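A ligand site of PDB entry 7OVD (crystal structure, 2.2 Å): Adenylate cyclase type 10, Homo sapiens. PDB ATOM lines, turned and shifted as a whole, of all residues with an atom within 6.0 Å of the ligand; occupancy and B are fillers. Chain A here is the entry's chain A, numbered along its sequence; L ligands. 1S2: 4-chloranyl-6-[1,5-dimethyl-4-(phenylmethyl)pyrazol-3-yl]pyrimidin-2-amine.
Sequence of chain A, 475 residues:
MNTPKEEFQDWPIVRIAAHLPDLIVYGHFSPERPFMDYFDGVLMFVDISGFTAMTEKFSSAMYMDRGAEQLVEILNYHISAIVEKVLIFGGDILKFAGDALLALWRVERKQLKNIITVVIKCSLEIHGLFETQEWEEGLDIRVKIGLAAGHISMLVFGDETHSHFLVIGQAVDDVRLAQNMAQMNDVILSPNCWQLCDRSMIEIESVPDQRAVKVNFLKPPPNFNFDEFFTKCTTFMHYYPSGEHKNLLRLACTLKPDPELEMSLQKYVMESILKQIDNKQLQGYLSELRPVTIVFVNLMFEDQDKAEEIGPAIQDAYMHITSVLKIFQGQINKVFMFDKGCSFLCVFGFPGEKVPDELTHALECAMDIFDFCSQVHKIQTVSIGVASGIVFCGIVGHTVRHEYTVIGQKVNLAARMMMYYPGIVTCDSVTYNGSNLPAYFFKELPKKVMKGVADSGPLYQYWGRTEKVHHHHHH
The backbone carbonyl oxygen (O) of Phe 165 is in hydrogen-bond range of the side-chain amino group (NZ) of Lys 95 (2.6 Å). The backbone carbonyl oxygen (O) of Lys 95 sits at hydrogen-bond distance from the backbone NH (N) of Leu 102 (3.2 Å). The backbone carbonyl oxygen (O) of Val 335 lies within hydrogen-bond range of the side-chain amino group (NZ) of Lys 95 (3.1 Å). The backbone NH (N) of Leu 94 is in hydrogen-bond range of the backbone carbonyl oxygen (O) of Leu 102 (2.6 Å). The side-chain amide oxygen of Gln 179 lies within hydrogen-bond range of the guanidinium group of Arg 176 (2.6 Å).
Merely in contact with the ligand: Phe 165 (3.2 Å), Phe 336 (3.3 Å), Leu 166 (3.5 Å), Lys 95 (3.5 Å), Phe 45 (3.5 Å), Phe 338 (3.6 Å), Leu 102 (3.6 Å), Val 172 (3.6 Å), Ala 97 (3.6 Å), Arg 176 (3.7 Å), Val 175 (3.7 Å), Ala 100 (3.7 Å), Phe 96 (3.8 Å) and Leu 101 (3.9 Å). Hydrophobic or aromatic side chains that line the ligand: Phe 45, Ala 97, Leu 102, Phe 165, Leu 166, Val 167, Val 172, Val 175, Phe 336, Met 337 and Phe 338. Within 4 Å of the ligand: Phe 45, Lys 95, Phe 96, Ala 97, Ala 100, Leu 101, Leu 102, Phe 165, Leu 166, Val 167, Val 172, Val 175, Arg 176, Phe 336, Met 337 and Phe 338.
N01 of the ligand sits at hydrogen-bond distance from N of Val 167 (3.0 Å). N22 of the ligand is in hydrogen-bond range of O of Val 167. N22 of the ligand sits at hydrogen-bond distance from O of Met 337, at 2.8 Å.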
ATOM      1  N   LEU A  23     -11.388 -10.705  23.944  1.00  0.00           N
ATOM      2  CA  LEU A  23     -12.127 -10.251  22.776  1.00  0.00           C
ATOM      3  C   LEU A  23     -12.005  -8.747  22.598  1.00  0.00           C
ATOM      4  O   LEU A  23     -11.856  -8.250  21.466  1.00  0.00           O
ATOM      5  CB  LEU A  23     -13.592 -10.651  22.941  1.00  0.00           C
ATOM      6  CG  LEU A  23     -14.535 -10.610  21.741  1.00  0.00           C
ATOM      7  CD1 LEU A  23     -14.134 -11.752  20.816  1.00  0.00           C
ATOM      8  CD2 LEU A  23     -15.971 -10.773  22.202  1.00  0.00           C
ATOM      9  N   PHE A  45     -22.209 -20.942  29.436  1.00  0.00           N
ATOM     10  CA  PHE A  45     -22.994 -20.120  30.344  1.00  0.00           C
ATOM     11  C   PHE A  45     -23.087 -20.835  31.685  1.00  0.00           C
ATOM     12  O   PHE A  45     -23.565 -21.972  31.733  1.00  0.00           O
ATOM     13  CB  PHE A  45     -24.386 -19.850  29.764  1.00  0.00           C
ATOM     14  CG  PHE A  45     -25.153 -18.794  30.508  1.00  0.00           C
ATOM     15  CD1 PHE A  45     -24.759 -17.460  30.443  1.00  0.00           C
ATOM     16  CD2 PHE A  45     -26.249 -19.127  31.280  1.00  0.00           C
ATOM     17  CE1 PHE A  45     -25.472 -16.475  31.128  1.00  0.00           C
ATOM     18  CE2 PHE A  45     -26.966 -18.137  31.976  1.00  0.00           C
ATOM     19  CZ  PHE A  45     -26.584 -16.819  31.889  1.00  0.00           C
ATOM     20  N   LEU A  94     -16.513 -13.382  29.153  1.00  0.00           N
ATOM     21  CA  LEU A  94     -16.981 -12.187  28.470  1.00  0.00           C
ATOM     22  C   LEU A  94     -17.642 -11.201  29.445  1.00  0.00           C
ATOM     23  O   LEU A  94     -17.292 -10.011  29.461  1.00  0.00           O
ATOM     24  CB  LEU A  94     -17.951 -12.567  27.339  1.00  0.00           C
ATOM     25  CG  LEU A  94     -17.372 -13.421  26.212  1.00  0.00           C
ATOM     26  CD1 LEU A  94     -18.456 -13.682  25.176  1.00  0.00           C
ATOM     27  CD2 LEU A  94     -16.110 -12.780  25.571  1.00  0.00           C
ATOM     28  N   LYS A  95     -18.601 -11.668  30.239  1.00  0.00           N
ATOM     29  CA  LYS A  95     -19.329 -10.753  31.096  1.00  0.00           C
ATOM     30  C   LYS A  95     -19.734 -11.497  32.343  1.00  0.00           C
ATOM     31  O   LYS A  95     -19.959 -12.704  32.310  1.00  0.00           O
ATOM     32  CB  LYS A  95     -20.592 -10.166  30.408  1.00  0.00           C
ATOM     33  CG  LYS A  95     -20.325  -8.852  29.668  1.00  0.00           C
ATOM     34  CD  LYS A  95     -21.547  -8.253  28.997  1.00  0.00           C
ATOM     35  CE  LYS A  95     -21.093  -7.377  27.831  1.00  0.00           C
ATOM     36  NZ  LYS A  95     -22.048  -6.308  27.402  1.00  0.00           N
ATOM     37  N   PHE A  96     -19.813 -10.763  33.456  1.00  0.00           N
ATOM     38  CA  PHE A  96     -20.402 -11.258  34.685  1.00  0.00           C
ATOM     39  C   PHE A  96     -21.746 -10.597  34.897  1.00  0.00           C
ATOM     40  O   PHE A  96     -21.952  -9.446  34.495  1.00  0.00           O
ATOM     41  CB  PHE A  96     -19.530 -10.935  35.898  1.00  0.00           C
ATOM     42  CG  PHE A  96     -18.207 -11.612  35.930  1.00  0.00           C
ATOM     43  CD1 PHE A  96     -17.123 -11.051  35.283  1.00  0.00           C
ATOM     44  CD2 PHE A  96     -18.012 -12.743  36.664  1.00  0.00           C
ATOM     45  CE1 PHE A  96     -15.874 -11.612  35.345  1.00  0.00           C
ATOM     46  CE2 PHE A  96     -16.749 -13.323  36.741  1.00  0.00           C
ATOM     47  CZ  PHE A  96     -15.677 -12.761  36.055  1.00  0.00           C
ATOM     48  N   ALA A  97     -22.649 -11.319  35.557  1.00  0.00           N
ATOM     49  CA  ALA A  97     -23.877 -10.724  36.062  1.00  0.00           C
ATOM     50  C   ALA A  97     -24.182 -11.388  37.384  1.00  0.00           C
ATOM     51  O   ALA A  97     -23.587 -12.421  37.715  1.00  0.00           O
ATOM     52  CB  ALA A  97     -25.044 -10.859  35.089  1.00  0.00           C
ATOM     53  N   ASP A  99     -26.285 -13.327  38.430  1.00  0.00           N
ATOM     54  CA  ASP A  99     -26.701 -14.730  38.403  1.00  0.00           C
ATOM     55  C   ASP A  99     -25.785 -15.666  37.624  1.00  0.00           C
ATOM     56  O   ASP A  99     -25.987 -16.874  37.712  1.00  0.00           O
ATOM     57  CB  ASP A  99     -28.133 -14.844  37.860  1.00  0.00           C
ATOM     58  CG  ASP A  99     -28.309 -14.250  36.454  1.00  0.00           C
ATOM     59  OD1 ASP A  99     -27.780 -13.156  36.178  1.00  0.00           O
ATOM     60  OD2 ASP A  99     -28.986 -14.883  35.614  1.00  0.00           O
ATOM     61  N   ALA A 100     -24.757 -15.175  36.889  1.00  0.00           N
ATOM     62  CA  ALA A 100     -24.118 -16.016  35.881  1.00  0.00           C
ATOM     63  C   ALA A 100     -22.824 -15.388  35.336  1.00  0.00           C
ATOM     64  O   ALA A 100     -22.493 -14.235  35.633  1.00  0.00           O
ATOM     65  CB  ALA A 100     -25.102 -16.274  34.733  1.00  0.00           C
ATOM     66  N   LEU A 101     -22.091 -16.161  34.535  1.00  0.00           N
ATOM     67  CA  LEU A 101     -21.067 -15.609  33.647  1.00  0.00           C
ATOM     68  C   LEU A 101     -21.102 -16.316  32.296  1.00  0.00           C
ATOM     69  O   LEU A 101     -21.524 -17.473  32.192  1.00  0.00           O
ATOM     70  CB  LEU A 101     -19.656 -15.672  34.273  1.00  0.00           C
ATOM     71  CG  LEU A 101     -18.891 -16.967  34.579  1.00  0.00           C
ATOM     72  CD1 LEU A 101     -18.147 -17.502  33.339  1.00  0.00           C
ATOM     73  CD2 LEU A 101     -17.913 -16.701  35.729  1.00  0.00           C
ATOM     74  N   LEU A 102     -20.641 -15.622  31.259  1.00  0.00           N
ATOM     75  CA  LEU A 102     -20.561 -16.165  29.905  1.00  0.00           C
ATOM     76  C   LEU A 102     -19.098 -16.205  29.466  1.00  0.00           C
ATOM     77  O   LEU A 102     -18.398 -15.188  29.536  1.00  0.00           O
ATOM     78  CB  LEU A 102     -21.403 -15.328  28.931  1.00  0.00           C
ATOM     79  CG  LEU A 102     -21.519 -15.720  27.462  1.00  0.00           C
ATOM     80  CD1 LEU A 102     -22.101 -17.127  27.268  1.00  0.00           C
ATOM     81  CD2 LEU A 102     -22.301 -14.701  26.647  1.00  0.00           C
ATOM     82  N   PHE A 165     -20.204  -3.942  24.376  1.00  0.00           N
ATOM     83  CA  PHE A 165     -20.146  -5.007  23.389  1.00  0.00           C
ATOM     84  C   PHE A 165     -21.173  -6.071  23.734  1.00  0.00           C
ATOM     85  O   PHE A 165     -21.649  -6.161  24.861  1.00  0.00           O
ATOM     86  CB  PHE A 165     -18.733  -5.615  23.271  1.00  0.00           C
ATOM     87  CG  PHE A 165     -18.310  -6.416  24.470  1.00  0.00           C
ATOM     88  CD1 PHE A 165     -17.763  -5.786  25.579  1.00  0.00           C
ATOM     89  CD2 PHE A 165     -18.444  -7.796  24.478  1.00  0.00           C
ATOM     90  CE1 PHE A 165     -17.376  -6.500  26.685  1.00  0.00           C
ATOM     91  CE2 PHE A 165     -18.061  -8.523  25.572  1.00  0.00           C
ATOM     92  CZ  PHE A 165     -17.541  -7.873  26.678  1.00  0.00           C
ATOM     93  N   LEU A 166     -21.480  -6.893  22.728  1.00  0.00           N
ATOM     94  CA  LEU A 166     -22.379  -8.021  22.853  1.00  0.00           C
ATOM     95  C   LEU A 166     -21.933  -9.105  21.883  1.00  0.00           C
ATOM     96  O   LEU A 166     -21.368  -8.801  20.825  1.00  0.00           O
ATOM     97  CB  LEU A 166     -23.824  -7.638  22.525  1.00  0.00           C
ATOM     98  CG  LEU A 166     -24.579  -6.828  23.560  1.00  0.00           C
ATOM     99  CD1 LEU A 166     -25.849  -6.284  22.915  1.00  0.00           C
ATOM    100  CD2 LEU A 166     -24.915  -7.714  24.763  1.00  0.00           C
ATOM    101  N   VAL A 167     -22.216 -10.347  22.208  1.00  0.00           N
ATOM    102  CA  VAL A 167     -22.182 -11.412  21.203  1.00  0.00           C
ATOM    103  C   VAL A 167     -23.621 -11.741  20.826  1.00  0.00           C
ATOM    104  O   VAL A 167     -24.512 -11.816  21.684  1.00  0.00           O
ATOM    105  CB  VAL A 167     -21.412 -12.668  21.669  1.00  0.00           C
ATOM    106  CG1 VAL A 167     -19.912 -12.393  21.744  1.00  0.00           C
ATOM    107  CG2 VAL A 167     -21.937 -13.204  22.997  1.00  0.00           C
ATOM    108  N   ILE A 168     -23.851 -11.918  19.531  1.00  0.00           N
ATOM    109  CA  ILE A 168     -25.182 -12.202  18.998  1.00  0.00           C
ATOM    110  C   ILE A 168     -25.077 -13.364  18.029  1.00  0.00           C
ATOM    111  O   ILE A 168     -24.014 -13.633  17.468  1.00  0.00           O
ATOM    112  CB  ILE A 168     -25.771 -10.946  18.318  1.00  0.00           C
ATOM    113  CG1 ILE A 168     -26.014  -9.868  19.358  1.00  0.00           C
ATOM    114  CG2 ILE A 168     -27.090 -11.224  17.652  1.00  0.00           C
ATOM    115  CD1 ILE A 168     -26.244  -8.510  18.730  1.00  0.00           C
ATOM    116  N   VAL A 172     -25.285 -18.017  20.577  1.00  0.00           N
ATOM    117  CA  VAL A 172     -25.725 -17.319  21.773  1.00  0.00           C
ATOM    118  C   VAL A 172     -27.131 -17.771  22.157  1.00  0.00           C
ATOM    119  O   VAL A 172     -27.397 -18.096  23.322  1.00  0.00           O
ATOM    120  CB  VAL A 172     -25.666 -15.795  21.584  1.00  0.00           C
ATOM    121  CG1 VAL A 172     -26.017 -15.120  22.878  1.00  0.00           C
ATOM    122  CG2 VAL A 172     -24.263 -15.369  21.144  1.00  0.00           C
ATOM    123  N   ASP A 173     -28.047 -17.809  21.195  1.00  0.00           N
ATOM    124  CA  ASP A 173     -29.379 -18.292  21.514  1.00  0.00           C
ATOM    125  C   ASP A 173     -29.349 -19.774  21.896  1.00  0.00           C
ATOM    126  O   ASP A 173     -30.050 -20.175  22.837  1.00  0.00           O
ATOM    127  CB  ASP A 173     -30.339 -18.028  20.346  1.00  0.00           C
ATOM    128  CG  ASP A 173     -30.566 -16.538  20.100  1.00  0.00           C
ATOM    129  OD1 ASP A 173     -30.670 -15.764  21.090  1.00  0.00           O
ATOM    130  OD2 ASP A 173     -30.645 -16.134  18.915  1.00  0.00           O
ATOM    131  N   VAL A 175     -26.916 -21.303  23.535  1.00  0.00           N
ATOM    132  CA  VAL A 175     -26.477 -21.428  24.927  1.00  0.00           C
ATOM    133  C   VAL A 175     -27.571 -20.929  25.840  1.00  0.00           C
ATOM    134  O   VAL A 175     -27.640 -21.335  26.999  1.00  0.00           O
ATOM    135  CB  VAL A 175     -25.126 -20.706  25.160  1.00  0.00           C
ATOM    136  CG1 VAL A 175     -25.338 -19.243  25.500  1.00  0.00           C
ATOM    137  CG2 VAL A 175     -24.326 -21.390  26.258  1.00  0.00           C
ATOM    138  N   ARG A 176     -28.474 -20.079  25.324  1.00  0.00           N
ATOM    139  CA  ARG A 176     -29.629 -19.626  26.091  1.00  0.00           C
ATOM    140  C   ARG A 176     -30.608 -20.766  26.325  1.00  0.00           C
ATOM    141  O   ARG A 176     -31.185 -20.869  27.410  1.00  0.00           O
ATOM    142  CB  ARG A 176     -30.322 -18.462  25.365  1.00  0.00           C
ATOM    143  CG  ARG A 176     -31.292 -17.623  26.214  1.00  0.00           C
ATOM    144  CD  ARG A 176     -32.650 -18.286  26.422  1.00  0.00           C
ATOM    145  NE  ARG A 176     -33.629 -17.445  27.088  1.00  0.00           N
ATOM    146  CZ  ARG A 176     -33.664 -17.213  28.391  1.00  0.00           C
ATOM    147  NH1 ARG A 176     -32.728 -17.667  29.200  1.00  0.00           N
ATOM    148  NH2 ARG A 176     -34.667 -16.502  28.903  1.00  0.00           N
ATOM    149  N   GLN A 179     -29.391 -23.270  28.694  1.00  0.00           N
ATOM    150  CA  GLN A 179     -29.507 -22.626  29.998  1.00  0.00           C
ATOM    151  C   GLN A 179     -30.804 -23.003  30.701  1.00  0.00           C
ATOM    152  O   GLN A 179     -30.837 -23.290  31.900  1.00  0.00           O
ATOM    153  CB  GLN A 179     -29.453 -21.098  29.831  1.00  0.00           C
ATOM    154  CG  GLN A 179     -29.336 -20.316  31.126  1.00  0.00           C
ATOM    155  CD  GLN A 179     -30.600 -19.603  31.564  1.00  0.00           C
ATOM    156  OE1 GLN A 179     -31.495 -19.322  30.760  1.00  0.00           O
ATOM    157  NE2 GLN A 179     -30.656 -19.290  32.843  1.00  0.00           N
ATOM    158  N   VAL A 335     -25.233  -4.524  29.762  1.00  0.00           N
ATOM    159  CA  VAL A 335     -26.022  -4.723  28.552  1.00  0.00           C
ATOM    160  C   VAL A 335     -26.012  -6.201  28.231  1.00  0.00           C
ATOM    161  O   VAL A 335     -24.956  -6.837  28.269  1.00  0.00           O
ATOM    162  CB  VAL A 335     -25.482  -3.927  27.352  1.00  0.00           C
ATOM    163  CG1 VAL A 335     -26.500  -4.054  26.191  1.00  0.00           C
ATOM    164  CG2 VAL A 335     -25.237  -2.475  27.723  1.00  0.00           C
ATOM    165  N   PHE A 336     -27.188  -6.753  27.898  1.00  0.00           N
ATOM    166  CA  PHE A 336     -27.264  -8.164  27.558  1.00  0.00           C
ATOM    167  C   PHE A 336     -28.053  -8.344  26.280  1.00  0.00           C
ATOM    168  O   PHE A 336     -28.718  -7.430  25.812  1.00  0.00           O
ATOM    169  CB  PHE A 336     -27.945  -8.984  28.646  1.00  0.00           C
ATOM    170  CG  PHE A 336     -27.362  -8.814  30.005  1.00  0.00           C
ATOM    171  CD1 PHE A 336     -26.072  -9.271  30.275  1.00  0.00           C
ATOM    172  CD2 PHE A 336     -28.116  -8.257  31.035  1.00  0.00           C
ATOM    173  CE1 PHE A 336     -25.526  -9.132  31.550  1.00  0.00           C
ATOM    174  CE2 PHE A 336     -27.588  -8.146  32.317  1.00  0.00           C
ATOM    175  CZ  PHE A 336     -26.297  -8.587  32.580  1.00  0.00           C
ATOM    176  N   MET A 337     -28.018  -9.562  25.718  1.00  0.00           N
ATOM    177  CA  MET A 337     -28.948  -9.861  24.638  1.00  0.00           C
ATOM    178  C   MET A 337     -29.175 -11.362  24.501  1.00  0.00           C
ATOM    179  O   MET A 337     -28.225 -12.139  24.484  1.00  0.00           O
ATOM    180  CB  MET A 337     -28.466  -9.318  23.306  1.00  0.00           C
ATOM    181  CG  MET A 337     -29.500  -9.511  22.206  1.00  0.00           C
ATOM    182  SD  MET A 337     -29.191  -8.396  20.832  1.00  0.00           S
ATOM    183  CE  MET A 337     -30.474  -8.906  19.691  1.00  0.00           C
ATOM    184  N   PHE A 338     -30.440 -11.752  24.371  1.00  0.00           N
ATOM    185  CA  PHE A 338     -30.836 -13.120  24.072  1.00  0.00           C
ATOM    186  C   PHE A 338     -32.328 -13.147  23.807  1.00  0.00           C
ATOM    187  O   PHE A 338     -33.074 -12.330  24.352  1.00  0.00           O
ATOM    188  CB  PHE A 338     -30.493 -14.080  25.210  1.00  0.00           C
ATOM    189  CG  PHE A 338     -31.138 -13.714  26.500  1.00  0.00           C
ATOM    190  CD1 PHE A 338     -30.536 -12.813  27.366  1.00  0.00           C
ATOM    191  CD2 PHE A 338     -32.346 -14.280  26.863  1.00  0.00           C
ATOM    192  CE1 PHE A 338     -31.130 -12.478  28.584  1.00  0.00           C
ATOM    193  CE2 PHE A 338     -32.950 -13.951  28.070  1.00  0.00           C
ATOM    194  CZ  PHE A 338     -32.342 -13.057  28.935  1.00  0.00           C
HETATM  195  C02 1S2 L   1     -24.745 -11.283  25.179  1.00  0.00           C
HETATM  196  C04 1S2 L   1     -24.225 -11.690  27.584  1.00  0.00           C
HETATM  197  C05 1S2 L   1     -22.829 -11.230  27.386  1.00  0.00           C
HETATM  198  C06 1S2 L   1     -22.440 -10.780  26.047  1.00  0.00           C
HETATM  199  C08 1S2 L   1     -25.514 -12.749  30.870  1.00  0.00           C
HETATM  200  C09 1S2 L   1     -25.764 -12.461  29.539  1.00  0.00           C
HETATM  201  C10 1S2 L   1     -24.574 -12.114  28.985  1.00  0.00           C
HETATM  202  C12 1S2 L   1     -27.989 -14.984  29.051  1.00  0.00           C
HETATM  203  C13 1S2 L   1     -28.144 -16.399  28.503  1.00  0.00           C
HETATM  204  C14 1S2 L   1     -27.596 -16.766  27.131  1.00  0.00           C
HETATM  205  C15 1S2 L   1     -26.876 -15.707  26.317  1.00  0.00           C
HETATM  206  C16 1S2 L   1     -26.713 -14.285  26.865  1.00  0.00           C
HETATM  207  C17 1S2 L   1     -27.255 -13.927  28.235  1.00  0.00           C
HETATM  208  C18 1S2 L   1     -23.431 -12.759  32.333  1.00  0.00           C
HETATM  209  C19 1S2 L   1     -26.561 -13.190  31.893  1.00  0.00           C
HETATM  210  C20 1S2 L   1     -27.105 -12.523  28.812  1.00  0.00           C
HETATM  211  N01 1S2 L   1     -23.382 -10.812  24.986  1.00  0.00           N
HETATM  212  N03 1S2 L   1     -25.156 -11.721  26.502  1.00  0.00           N
HETATM  213  N07 1S2 L   1     -24.198 -12.567  31.111  1.00  0.00           N
HETATM  214  N11 1S2 L   1     -23.627 -12.183  29.914  1.00  0.00           N
HETATM  215  N22 1S2 L   1     -25.637 -11.313  24.052  1.00  0.00           N
HETATM  216 CL1  1S2 L   1     -20.834 -10.193  25.625  1.00  0.00          CL
